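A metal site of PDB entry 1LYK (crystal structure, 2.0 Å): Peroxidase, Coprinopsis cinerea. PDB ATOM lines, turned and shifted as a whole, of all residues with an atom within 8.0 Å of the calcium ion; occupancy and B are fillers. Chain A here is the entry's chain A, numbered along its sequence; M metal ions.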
ATOM      1  N   PRO A 129      15.816 -14.531 -14.209  1.00  0.00           N
ATOM      2  CA  PRO A 129      15.115 -13.467 -13.477  1.00  0.00           C
ATOM      3  C   PRO A 129      16.086 -12.560 -12.722  1.00  0.00           C
ATOM      4  O   PRO A 129      17.059 -13.029 -12.130  1.00  0.00           O
ATOM      5  CB  PRO A 129      14.232 -14.257 -12.515  1.00  0.00           C
ATOM      6  CG  PRO A 129      13.863 -15.455 -13.317  1.00  0.00           C
ATOM      7  CD  PRO A 129      15.183 -15.838 -13.950  1.00  0.00           C
ATOM      8  N   ALA A 181      29.548 -10.476  -9.937  1.00  0.00           N
ATOM      9  CA  ALA A 181      28.117 -10.659  -9.681  1.00  0.00           C
ATOM     10  C   ALA A 181      27.659 -11.913 -10.437  1.00  0.00           C
ATOM     11  O   ALA A 181      26.679 -12.549 -10.056  1.00  0.00           O
ATOM     12  CB  ALA A 181      27.354  -9.468 -10.141  1.00  0.00           C
ATOM     13  N   ALA A 182      28.383 -12.263 -11.496  1.00  0.00           N
ATOM     14  CA  ALA A 182      28.051 -13.440 -12.307  1.00  0.00           C
ATOM     15  C   ALA A 182      28.020 -14.709 -11.475  1.00  0.00           C
ATOM     16  O   ALA A 182      27.375 -15.683 -11.856  1.00  0.00           O
ATOM     17  CB  ALA A 182      29.037 -13.589 -13.456  1.00  0.00           C
ATOM     18  N   HIS A 183      28.726 -14.715 -10.338  1.00  0.00           N
ATOM     19  CA  HIS A 183      28.724 -15.886  -9.460  1.00  0.00           C
ATOM     20  C   HIS A 183      27.376 -16.099  -8.754  1.00  0.00           C
ATOM     21  O   HIS A 183      27.176 -17.083  -8.041  1.00  0.00           O
ATOM     22  CB  HIS A 183      29.872 -15.855  -8.455  1.00  0.00           C
ATOM     23  CG  HIS A 183      31.203 -16.332  -9.032  1.00  0.00           C
ATOM     24  ND1 HIS A 183      32.368 -16.638  -8.321  1.00  0.00           N
ATOM     25  CD2 HIS A 183      31.448 -16.538 -10.380  1.00  0.00           C
ATOM     26  CE1 HIS A 183      33.300 -16.950  -9.211  1.00  0.00           C
ATOM     27  NE2 HIS A 183      32.774 -16.930 -10.404  1.00  0.00           N
ATOM     28  N   SER A 184      26.438 -15.170  -9.001  1.00  0.00           N
ATOM     29  CA  SER A 184      25.101 -15.287  -8.439  1.00  0.00           C
ATOM     30  C   SER A 184      24.268 -16.280  -9.267  1.00  0.00           C
ATOM     31  O   SER A 184      23.122 -16.607  -8.881  1.00  0.00           O
ATOM     32  CB  SER A 184      24.409 -13.928  -8.392  1.00  0.00           C
ATOM     33  OG  SER A 184      23.109 -14.068  -7.836  1.00  0.00           O
ATOM     34  N   LEU A 185      24.816 -16.713 -10.396  1.00  0.00           N
ATOM     35  CA  LEU A 185      24.182 -17.700 -11.275  1.00  0.00           C
ATOM     36  C   LEU A 185      25.311 -18.705 -11.536  1.00  0.00           C
ATOM     37  O   LEU A 185      25.727 -18.902 -12.679  1.00  0.00           O
ATOM     38  CB  LEU A 185      23.788 -17.030 -12.600  1.00  0.00           C
ATOM     39  CG  LEU A 185      22.786 -15.875 -12.653  1.00  0.00           C
ATOM     40  CD1 LEU A 185      22.789 -15.237 -14.026  1.00  0.00           C
ATOM     41  CD2 LEU A 185      21.404 -16.397 -12.328  1.00  0.00           C
ATOM     42  N   ALA A 186      25.760 -19.383 -10.482  1.00  0.00           N
ATOM     43  CA  ALA A 186      26.899 -20.279 -10.621  1.00  0.00           C
ATOM     44  C   ALA A 186      26.958 -21.498  -9.727  1.00  0.00           C
ATOM     45  O   ALA A 186      26.360 -21.536  -8.647  1.00  0.00           O
ATOM     46  CB  ALA A 186      28.188 -19.475 -10.447  1.00  0.00           C
ATOM     47  N   LEU A 200      26.944 -21.635  -5.828  1.00  0.00           N
ATOM     48  CA  LEU A 200      27.797 -20.651  -5.170  1.00  0.00           C
ATOM     49  C   LEU A 200      26.921 -19.720  -4.303  1.00  0.00           C
ATOM     50  O   LEU A 200      27.443 -18.989  -3.464  1.00  0.00           O
ATOM     51  CB  LEU A 200      28.620 -19.886  -6.211  1.00  0.00           C
ATOM     52  CG  LEU A 200      30.082 -20.307  -6.447  1.00  0.00           C
ATOM     53  CD1 LEU A 200      30.262 -21.814  -6.563  1.00  0.00           C
ATOM     54  CD2 LEU A 200      30.602 -19.614  -7.686  1.00  0.00           C
ATOM     55  N   ASP A 201      25.620 -19.696  -4.551  1.00  0.00           N
ATOM     56  CA  ASP A 201      24.692 -18.913  -3.719  1.00  0.00           C
ATOM     57  C   ASP A 201      23.380 -19.686  -3.675  1.00  0.00           C
ATOM     58  O   ASP A 201      23.213 -20.625  -4.451  1.00  0.00           O
ATOM     59  CB  ASP A 201      24.569 -17.427  -4.140  1.00  0.00           C
ATOM     60  CG  ASP A 201      23.622 -17.156  -5.298  1.00  0.00           C
ATOM     61  OD1 ASP A 201      23.056 -18.080  -5.907  1.00  0.00           O
ATOM     62  OD2 ASP A 201      23.423 -15.975  -5.604  1.00  0.00           O
ATOM     63  N   SER A 202      22.452 -19.313  -2.813  1.00  0.00           N
ATOM     64  CA  SER A 202      21.214 -20.088  -2.690  1.00  0.00           C
ATOM     65  C   SER A 202      20.265 -20.017  -3.875  1.00  0.00           C
ATOM     66  O   SER A 202      19.330 -20.794  -3.965  1.00  0.00           O
ATOM     67  CB  SER A 202      20.484 -19.703  -1.411  1.00  0.00           C
ATOM     68  OG  SER A 202      20.218 -18.313  -1.403  1.00  0.00           O
ATOM     69  N   THR A 203      20.528 -19.099  -4.809  1.00  0.00           N
ATOM     70  CA  THR A 203      19.688 -18.927  -5.985  1.00  0.00           C
ATOM     71  C   THR A 203      20.492 -18.948  -7.306  1.00  0.00           C
ATOM     72  O   THR A 203      20.742 -17.890  -7.900  1.00  0.00           O
ATOM     73  CB  THR A 203      18.922 -17.604  -5.867  1.00  0.00           C
ATOM     74  OG1 THR A 203      19.859 -16.519  -5.745  1.00  0.00           O
ATOM     75  CG2 THR A 203      18.025 -17.617  -4.626  1.00  0.00           C
ATOM     76  N   PRO A 204      20.931 -20.130  -7.751  1.00  0.00           N
ATOM     77  CA  PRO A 204      21.710 -20.270  -8.992  1.00  0.00           C
ATOM     78  C   PRO A 204      20.978 -19.922 -10.285  1.00  0.00           C
ATOM     79  O   PRO A 204      21.593 -19.861 -11.352  1.00  0.00           O
ATOM     80  CB  PRO A 204      22.143 -21.730  -8.953  1.00  0.00           C
ATOM     81  CG  PRO A 204      20.981 -22.391  -8.248  1.00  0.00           C
ATOM     82  CD  PRO A 204      20.743 -21.438  -7.110  1.00  0.00           C
ATOM     83  N   GLN A 205      19.677 -19.696 -10.200  1.00  0.00           N
ATOM     84  CA  GLN A 205      18.876 -19.321 -11.370  1.00  0.00           C
ATOM     85  C   GLN A 205      18.307 -17.913 -11.217  1.00  0.00           C
ATOM     86  O   GLN A 205      17.433 -17.502 -11.985  1.00  0.00           O
ATOM     87  CB  GLN A 205      17.735 -20.321 -11.586  1.00  0.00           C
ATOM     88  CG  GLN A 205      18.203 -21.737 -11.827  1.00  0.00           C
ATOM     89  CD  GLN A 205      17.078 -22.652 -12.278  1.00  0.00           C
ATOM     90  OE1 GLN A 205      16.372 -23.251 -11.466  1.00  0.00           O
ATOM     91  NE2 GLN A 205      16.916 -22.765 -13.593  1.00  0.00           N
ATOM     92  N   VAL A 206      18.799 -17.149 -10.246  1.00  0.00           N
ATOM     93  CA  VAL A 206      18.317 -15.788 -10.026  1.00  0.00           C
ATOM     94  C   VAL A 206      19.508 -14.847  -9.868  1.00  0.00           C
ATOM     95  O   VAL A 206      20.377 -15.034  -8.988  1.00  0.00           O
ATOM     96  CB  VAL A 206      17.396 -15.679  -8.763  1.00  0.00           C
ATOM     97  CG1 VAL A 206      16.767 -14.295  -8.689  1.00  0.00           C
ATOM     98  CG2 VAL A 206      16.310 -16.750  -8.764  1.00  0.00           C
ATOM     99  N   PHE A 207      19.571 -13.853 -10.731  1.00  0.00           N
ATOM    100  CA  PHE A 207      20.638 -12.873 -10.687  1.00  0.00           C
ATOM    101  C   PHE A 207      20.249 -11.885  -9.605  1.00  0.00           C
ATOM    102  O   PHE A 207      19.518 -10.942  -9.857  1.00  0.00           O
ATOM    103  CB  PHE A 207      20.767 -12.155 -12.033  1.00  0.00           C
ATOM    104  CG  PHE A 207      22.004 -11.317 -12.149  1.00  0.00           C
ATOM    105  CD1 PHE A 207      23.257 -11.910 -12.222  1.00  0.00           C
ATOM    106  CD2 PHE A 207      21.917  -9.926 -12.142  1.00  0.00           C
ATOM    107  CE1 PHE A 207      24.405 -11.146 -12.304  1.00  0.00           C
ATOM    108  CE2 PHE A 207      23.065  -9.142 -12.212  1.00  0.00           C
ATOM    109  CZ  PHE A 207      24.306  -9.751 -12.296  1.00  0.00           C
ATOM    110  N   ASP A 208      20.770 -12.102  -8.402  1.00  0.00           N
ATOM    111  CA  ASP A 208      20.462 -11.271  -7.249  1.00  0.00           C
ATOM    112  C   ASP A 208      21.705 -11.097  -6.385  1.00  0.00           C
ATOM    113  O   ASP A 208      22.771 -11.650  -6.709  1.00  0.00           O
ATOM    114  CB  ASP A 208      19.357 -11.929  -6.414  1.00  0.00           C
ATOM    115  CG  ASP A 208      19.666 -13.390  -6.097  1.00  0.00           C
ATOM    116  OD1 ASP A 208      20.804 -13.815  -6.339  1.00  0.00           O
ATOM    117  OD2 ASP A 208      18.773 -14.106  -5.605  1.00  0.00           O
ATOM    118  N   THR A 209      21.563 -10.418  -5.249  1.00  0.00           N
ATOM    119  CA  THR A 209      22.668 -10.149  -4.352  1.00  0.00           C
ATOM    120  C   THR A 209      23.017 -11.264  -3.369  1.00  0.00           C
ATOM    121  O   THR A 209      23.990 -11.151  -2.619  1.00  0.00           O
ATOM    122  CB  THR A 209      22.440  -8.852  -3.567  1.00  0.00           C
ATOM    123  OG1 THR A 209      21.274  -8.996  -2.743  1.00  0.00           O
ATOM    124  CG2 THR A 209      22.237  -7.688  -4.518  1.00  0.00           C
ATOM    125  N   GLN A 210      22.264 -12.362  -3.393  1.00  0.00           N
ATOM    126  CA  GLN A 210      22.550 -13.470  -2.480  1.00  0.00           C
ATOM    127  C   GLN A 210      24.023 -13.902  -2.464  1.00  0.00           C
ATOM    128  O   GLN A 210      24.560 -14.208  -1.414  1.00  0.00           O
ATOM    129  CB  GLN A 210      21.640 -14.676  -2.770  1.00  0.00           C
ATOM    130  CG  GLN A 210      20.173 -14.442  -2.470  1.00  0.00           C
ATOM    131  CD  GLN A 210      19.935 -13.817  -1.107  1.00  0.00           C
ATOM    132  OE1 GLN A 210      19.219 -12.817  -0.988  1.00  0.00           O
ATOM    133  NE2 GLN A 210      20.530 -14.389  -0.079  1.00  0.00           N
ATOM    134  N   PHE A 211      24.687 -13.893  -3.616  1.00  0.00           N
ATOM    135  CA  PHE A 211      26.093 -14.286  -3.663  1.00  0.00           C
ATOM    136  C   PHE A 211      26.948 -13.432  -2.738  1.00  0.00           C
ATOM    137  O   PHE A 211      27.766 -13.946  -1.960  1.00  0.00           O
ATOM    138  CB  PHE A 211      26.633 -14.193  -5.107  1.00  0.00           C
ATOM    139  CG  PHE A 211      28.143 -14.261  -5.206  1.00  0.00           C
ATOM    140  CD1 PHE A 211      28.815 -15.459  -4.988  1.00  0.00           C
ATOM    141  CD2 PHE A 211      28.894 -13.127  -5.508  1.00  0.00           C
ATOM    142  CE1 PHE A 211      30.195 -15.519  -5.069  1.00  0.00           C
ATOM    143  CE2 PHE A 211      30.280 -13.168  -5.585  1.00  0.00           C
ATOM    144  CZ  PHE A 211      30.936 -14.371  -5.367  1.00  0.00           C
ATOM    145  N   TYR A 212      26.759 -12.113  -2.778  1.00  0.00           N
ATOM    146  CA  TYR A 212      27.557 -11.228  -1.947  1.00  0.00           C
ATOM    147  C   TYR A 212      27.278 -11.379  -0.467  1.00  0.00           C
ATOM    148  O   TYR A 212      28.181 -11.292   0.356  1.00  0.00           O
ATOM    149  CB  TYR A 212      27.365  -9.789  -2.386  1.00  0.00           C
ATOM    150  CG  TYR A 212      27.900  -9.543  -3.778  1.00  0.00           C
ATOM    151  CD1 TYR A 212      29.241  -9.245  -3.975  1.00  0.00           C
ATOM    152  CD2 TYR A 212      27.059  -9.595  -4.885  1.00  0.00           C
ATOM    153  CE1 TYR A 212      29.733  -8.962  -5.234  1.00  0.00           C
ATOM    154  CE2 TYR A 212      27.541  -9.314  -6.166  1.00  0.00           C
ATOM    155  CZ  TYR A 212      28.875  -8.999  -6.330  1.00  0.00           C
ATOM    156  OH  TYR A 212      29.370  -8.688  -7.575  1.00  0.00           O
ATOM    157  N   GLU A 214      25.868 -14.209   1.104  1.00  0.00           N
ATOM    158  CA  GLU A 214      26.283 -15.528   1.572  1.00  0.00           C
ATOM    159  C   GLU A 214      27.772 -15.801   1.670  1.00  0.00           C
ATOM    160  O   GLU A 214      28.204 -16.548   2.540  1.00  0.00           O
ATOM    161  CB  GLU A 214      25.523 -16.602   0.789  1.00  0.00           C
ATOM    162  CG  GLU A 214      24.023 -16.469   1.013  1.00  0.00           C
ATOM    163  CD  GLU A 214      23.174 -17.242   0.020  1.00  0.00           C
ATOM    164  OE1 GLU A 214      22.017 -16.826  -0.169  1.00  0.00           O
ATOM    165  OE2 GLU A 214      23.641 -18.241  -0.548  1.00  0.00           O
ATOM    166  N   ASN A 265      19.464  -5.038  -5.561  1.00  0.00           N
ATOM    167  CA  ASN A 265      19.597  -5.811  -6.793  1.00  0.00           C
ATOM    168  C   ASN A 265      19.788  -4.883  -7.979  1.00  0.00           C
ATOM    169  O   ASN A 265      20.520  -5.200  -8.913  1.00  0.00           O
ATOM    170  CB  ASN A 265      18.369  -6.693  -7.001  1.00  0.00           C
ATOM    171  CG  ASN A 265      18.398  -7.947  -6.144  1.00  0.00           C
ATOM    172  OD1 ASN A 265      19.433  -8.598  -6.019  1.00  0.00           O
ATOM    173  ND2 ASN A 265      17.256  -8.293  -5.552  1.00  0.00           N
ATOM    174  N   MET A 268      23.469  -3.546  -8.089  1.00  0.00           N
ATOM    175  CA  MET A 268      24.338  -4.633  -8.521  1.00  0.00           C
ATOM    176  C   MET A 268      24.222  -4.802 -10.033  1.00  0.00           C
ATOM    177  O   MET A 268      25.229  -4.848 -10.742  1.00  0.00           O
ATOM    178  CB  MET A 268      23.947  -5.939  -7.820  1.00  0.00           C
ATOM    179  CG  MET A 268      24.780  -7.138  -8.236  1.00  0.00           C
ATOM    180  SD  MET A 268      24.140  -8.713  -7.628  1.00  0.00           S
ATOM    181  CE  MET A 268      22.756  -8.902  -8.670  1.00  0.00           C
ATOM    182  N   ASN A 302      12.655  -9.685 -10.721  1.00  0.00           N
ATOM    183  CA  ASN A 302      12.906 -10.422  -9.491  1.00  0.00           C
ATOM    184  C   ASN A 302      12.498  -9.452  -8.399  1.00  0.00           C
ATOM    185  O   ASN A 302      13.128  -8.405  -8.211  1.00  0.00           O
ATOM    186  CB  ASN A 302      14.389 -10.759  -9.299  1.00  0.00           C
ATOM    187  CG  ASN A 302      14.689 -11.303  -7.905  1.00  0.00           C
ATOM    188  OD1 ASN A 302      15.737 -11.011  -7.331  1.00  0.00           O
ATOM    189  ND2 ASN A 302      13.787 -12.104  -7.361  1.00  0.00           N
HETATM  190 CA    CA M   1      21.731 -15.905  -7.302  1.00  0.00          CA
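Within 4 Å of the calcium ion: Ser 184, Asp 201, Thr 203, Val 206 and Asp 208.
The nearest printed residue that does not touch the calcium ion is Pro 204 (4.3 Å).
The calcium ion is bound by O of Ser 184 (2.2 Å), O of Thr 203 (2.3 Å), O of Val 206 (2.3 Å), OG of Ser 184 (2.4 Å), OD2 of Asp 201 (2.4 Å), OD1 of Asp 208 (2.5 Å) and OG1 of Thr 203 (2.5 Å).
Slightly farther from the calcium ion lies OD1 of Asp 201 (2.9 Å).
The backbone NH (N) of Phe 211 sits close to the side-chain carboxylate (OD2) of Asp 201, at 3.1 Å.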
